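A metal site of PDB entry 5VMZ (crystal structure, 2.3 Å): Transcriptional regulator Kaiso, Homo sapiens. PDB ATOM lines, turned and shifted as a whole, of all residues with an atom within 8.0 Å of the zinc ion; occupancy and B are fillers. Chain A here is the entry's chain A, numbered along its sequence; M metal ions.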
ATOM      1  N   GLN A  81     -23.261   6.018   0.881  1.00  0.00           N
ATOM      2  CA  GLN A  81     -24.618   5.579   1.203  1.00  0.00           C
ATOM      3  C   GLN A  81     -24.879   4.132   0.774  1.00  0.00           C
ATOM      4  O   GLN A  81     -24.686   3.776  -0.380  1.00  0.00           O
ATOM      5  CB  GLN A  81     -25.664   6.504   0.557  1.00  0.00           C
ATOM      6  CG  GLN A  81     -27.114   6.135   0.943  1.00  0.00           C
ATOM      7  CD  GLN A  81     -28.109   7.125   0.391  1.00  0.00           C
ATOM      8  OE1 GLN A  81     -27.838   7.805  -0.597  1.00  0.00           O
ATOM      9  NE2 GLN A  81     -29.276   7.224   1.043  1.00  0.00           N
ATOM     10  N   CYS A  82     -25.307   3.312   1.724  1.00  0.00           N
ATOM     11  CA  CYS A  82     -25.724   1.947   1.421  1.00  0.00           C
ATOM     12  C   CYS A  82     -26.990   1.957   0.556  1.00  0.00           C
ATOM     13  O   CYS A  82     -28.008   2.539   0.946  1.00  0.00           O
ATOM     14  CB  CYS A  82     -25.962   1.167   2.712  1.00  0.00           C
ATOM     15  SG  CYS A  82     -26.715  -0.450   2.449  1.00  0.00           S
ATOM     16  N   LEU A  83     -26.909   1.328  -0.614  1.00  0.00           N
ATOM     17  CA  LEU A  83     -28.019   1.341  -1.542  1.00  0.00           C
ATOM     18  C   LEU A  83     -29.047   0.276  -1.203  1.00  0.00           C
ATOM     19  O   LEU A  83     -30.112   0.238  -1.790  1.00  0.00           O
ATOM     20  CB  LEU A  83     -27.542   1.149  -2.978  1.00  0.00           C
ATOM     21  CG  LEU A  83     -26.824   2.358  -3.594  1.00  0.00           C
ATOM     22  CD1 LEU A  83     -26.480   2.099  -5.044  1.00  0.00           C
ATOM     23  CD2 LEU A  83     -27.696   3.601  -3.456  1.00  0.00           C
ATOM     24  N   ALA A  84     -28.737  -0.587  -0.247  1.00  0.00           N
ATOM     25  CA  ALA A  84     -29.713  -1.612   0.135  1.00  0.00           C
ATOM     26  C   ALA A  84     -30.767  -1.099   1.141  1.00  0.00           C
ATOM     27  O   ALA A  84     -31.914  -1.536   1.097  1.00  0.00           O
ATOM     28  CB  ALA A  84     -29.008  -2.851   0.692  1.00  0.00           C
ATOM     29  N   CYS A  85     -30.373  -0.193   2.036  1.00  0.00           N
ATOM     30  CA  CYS A  85     -31.306   0.286   3.075  1.00  0.00           C
ATOM     31  C   CYS A  85     -31.301   1.808   3.240  1.00  0.00           C
ATOM     32  O   CYS A  85     -32.129   2.369   3.960  1.00  0.00           O
ATOM     33  CB  CYS A  85     -30.988  -0.358   4.418  1.00  0.00           C
ATOM     34  SG  CYS A  85     -29.424   0.210   5.129  1.00  0.00           S
ATOM     35  N   GLY A  86     -30.348   2.478   2.594  1.00  0.00           N
ATOM     36  CA  GLY A  86     -30.304   3.926   2.580  1.00  0.00           C
ATOM     37  C   GLY A  86     -29.388   4.604   3.601  1.00  0.00           C
ATOM     38  O   GLY A  86     -29.181   5.812   3.542  1.00  0.00           O
ATOM     39  N   LYS A  87     -28.872   3.830   4.563  1.00  0.00           N
ATOM     40  CA  LYS A  87     -27.985   4.372   5.590  1.00  0.00           C
ATOM     41  C   LYS A  87     -26.748   4.994   4.991  1.00  0.00           C
ATOM     42  O   LYS A  87     -26.140   4.429   4.062  1.00  0.00           O
ATOM     43  CB  LYS A  87     -27.540   3.287   6.584  1.00  0.00           C
ATOM     44  CG  LYS A  87     -28.491   3.040   7.746  1.00  0.00           C
ATOM     45  CD  LYS A  87     -27.692   2.599   8.957  1.00  0.00           C
ATOM     46  CE  LYS A  87     -28.566   2.413  10.178  1.00  0.00           C
ATOM     47  NZ  LYS A  87     -29.601   1.387   9.914  1.00  0.00           N
ATOM     48  N   SER A  88     -26.345   6.125   5.541  1.00  0.00           N
ATOM     49  CA  SER A  88     -25.115   6.782   5.093  1.00  0.00           C
ATOM     50  C   SER A  88     -23.962   6.710   6.103  1.00  0.00           C
ATOM     51  O   SER A  88     -24.191   6.635   7.307  1.00  0.00           O
ATOM     52  CB  SER A  88     -25.416   8.235   4.754  1.00  0.00           C
ATOM     53  OG  SER A  88     -26.376   8.308   3.731  1.00  0.00           O
ATOM     54  N   PHE A  89     -22.733   6.776   5.592  1.00  0.00           N
ATOM     55  CA  PHE A  89     -21.528   6.600   6.411  1.00  0.00           C
ATOM     56  C   PHE A  89     -20.488   7.645   6.032  1.00  0.00           C
ATOM     57  O   PHE A  89     -20.511   8.171   4.902  1.00  0.00           O
ATOM     58  CB  PHE A  89     -21.000   5.170   6.252  1.00  0.00           C
ATOM     59  CG  PHE A  89     -22.035   4.147   6.565  1.00  0.00           C
ATOM     60  CD1 PHE A  89     -22.222   3.708   7.868  1.00  0.00           C
ATOM     61  CD2 PHE A  89     -22.920   3.720   5.579  1.00  0.00           C
ATOM     62  CE1 PHE A  89     -23.229   2.809   8.181  1.00  0.00           C
ATOM     63  CE2 PHE A  89     -23.938   2.813   5.889  1.00  0.00           C
ATOM     64  CZ  PHE A  89     -24.088   2.359   7.185  1.00  0.00           C
ATOM     65  N   MET A  95     -18.983   1.997   5.762  1.00  0.00           N
ATOM     66  CA  MET A  95     -19.943   1.574   4.741  1.00  0.00           C
ATOM     67  C   MET A  95     -19.747   0.085   4.434  1.00  0.00           C
ATOM     68  O   MET A  95     -20.724  -0.671   4.413  1.00  0.00           O
ATOM     69  CB  MET A  95     -19.768   2.405   3.461  1.00  0.00           C
ATOM     70  CG  MET A  95     -20.568   1.926   2.238  1.00  0.00           C
ATOM     71  SD  MET A  95     -19.878   0.502   1.323  1.00  0.00           S
ATOM     72  CE  MET A  95     -18.306   1.159   0.755  1.00  0.00           C
ATOM     73  N   HIS A  98     -20.689  -2.210   7.307  1.00  0.00           N
ATOM     74  CA  HIS A  98     -22.143  -2.288   7.415  1.00  0.00           C
ATOM     75  C   HIS A  98     -22.724  -3.290   6.435  1.00  0.00           C
ATOM     76  O   HIS A  98     -23.515  -4.150   6.799  1.00  0.00           O
ATOM     77  CB  HIS A  98     -22.767  -0.907   7.180  1.00  0.00           C
ATOM     78  CG  HIS A  98     -24.223  -0.967   6.836  1.00  0.00           C
ATOM     79  ND1 HIS A  98     -25.217  -1.059   7.791  1.00  0.00           N
ATOM     80  CD2 HIS A  98     -24.863  -0.990   5.638  1.00  0.00           C
ATOM     81  CE1 HIS A  98     -26.398  -1.119   7.204  1.00  0.00           C
ATOM     82  NE2 HIS A  98     -26.209  -1.085   5.892  1.00  0.00           N
ATOM     83  N   ILE A  99     -22.313  -3.177   5.178  1.00  0.00           N
ATOM     84  CA  ILE A  99     -22.904  -3.982   4.131  1.00  0.00           C
ATOM     85  C   ILE A  99     -22.532  -5.450   4.320  1.00  0.00           C
ATOM     86  O   ILE A  99     -23.393  -6.337   4.147  1.00  0.00           O
ATOM     87  CB  ILE A  99     -22.479  -3.455   2.756  1.00  0.00           C
ATOM     88  CG1 ILE A  99     -23.160  -2.101   2.505  1.00  0.00           C
ATOM     89  CG2 ILE A  99     -22.903  -4.402   1.656  1.00  0.00           C
ATOM     90  CD1 ILE A  99     -22.835  -1.505   1.141  1.00  0.00           C
ATOM     91  N   LYS A 100     -21.291  -5.724   4.719  1.00  0.00           N
ATOM     92  CA  LYS A 100     -20.867  -7.091   4.962  1.00  0.00           C
ATOM     93  C   LYS A 100     -21.631  -7.679   6.136  1.00  0.00           C
ATOM     94  O   LYS A 100     -22.105  -8.808   6.083  1.00  0.00           O
ATOM     95  CB  LYS A 100     -19.353  -7.183   5.215  1.00  0.00           C
ATOM     96  CG  LYS A 100     -18.476  -6.959   3.976  1.00  0.00           C
ATOM     97  CD  LYS A 100     -16.951  -7.049   4.314  1.00  0.00           C
ATOM     98  CE  LYS A 100     -16.086  -6.833   3.072  1.00  0.00           C
ATOM     99  NZ  LYS A 100     -14.607  -6.843   3.357  1.00  0.00           N
ATOM    100  N   VAL A 102     -24.561  -6.367   7.832  1.00  0.00           N
ATOM    101  CA  VAL A 102     -26.023  -6.324   7.813  1.00  0.00           C
ATOM    102  C   VAL A 102     -26.599  -7.001   6.577  1.00  0.00           C
ATOM    103  O   VAL A 102     -27.606  -7.696   6.643  1.00  0.00           O
ATOM    104  CB  VAL A 102     -26.546  -4.868   7.897  1.00  0.00           C
ATOM    105  CG1 VAL A 102     -28.104  -4.830   7.851  1.00  0.00           C
ATOM    106  CG2 VAL A 102     -26.059  -4.214   9.185  1.00  0.00           C
ATOM    107  N   HIS A 103     -25.931  -6.825   5.431  1.00  0.00           N
ATOM    108  CA  HIS A 103     -26.484  -7.330   4.180  1.00  0.00           C
ATOM    109  C   HIS A 103     -25.766  -8.579   3.615  1.00  0.00           C
ATOM    110  O   HIS A 103     -26.172  -9.101   2.582  1.00  0.00           O
ATOM    111  CB  HIS A 103     -26.479  -6.199   3.150  1.00  0.00           C
ATOM    112  CG  HIS A 103     -27.307  -5.028   3.567  1.00  0.00           C
ATOM    113  ND1 HIS A 103     -28.633  -5.143   3.930  1.00  0.00           N
ATOM    114  CD2 HIS A 103     -27.003  -3.715   3.678  1.00  0.00           C
ATOM    115  CE1 HIS A 103     -29.103  -3.953   4.254  1.00  0.00           C
ATOM    116  NE2 HIS A 103     -28.138  -3.063   4.112  1.00  0.00           N
ATOM    117  N   LEU A 113     -23.582  -1.486  -5.011  1.00  0.00           N
ATOM    118  CA  LEU A 113     -24.173  -1.647  -3.673  1.00  0.00           C
ATOM    119  C   LEU A 113     -24.108  -0.357  -2.840  1.00  0.00           C
ATOM    120  O   LEU A 113     -24.830  -0.211  -1.851  1.00  0.00           O
ATOM    121  CB  LEU A 113     -23.479  -2.780  -2.917  1.00  0.00           C
ATOM    122  CG  LEU A 113     -23.583  -4.201  -3.507  1.00  0.00           C
ATOM    123  CD1 LEU A 113     -22.677  -5.186  -2.766  1.00  0.00           C
ATOM    124  CD2 LEU A 113     -25.036  -4.687  -3.494  1.00  0.00           C
HETATM  125 ZN    ZN M   1     -27.587  -1.027   4.392  1.00  0.00          ZN
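The side-chain sulfur (SG) of Cys 82 lies close to the backbone NH (N) of Ala 84 (3.4 Å).
N of Cys 82 lies within hydrogen-bond range of O of Lys 87 (2.7 Å).
The side-chain sulfur (SG) of Cys 85 lies close to the backbone NH (N) of Lys 87 (3.7 Å).
Four residues have an atom within 4 Å of the zinc ion: Cys 82, Cys 85, His 98 and His 103.
The zinc ion is bound by NE2 of His 98.
The zinc ion is bound by NE2 of His 103 (2.1 Å).
SG of Cys 82 binds the zinc ion, 2.2 Å away.
The zinc ion is bound by SG of Cys 85 (2.3 Å).
The zinc ion has four donor atoms within binding distance.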
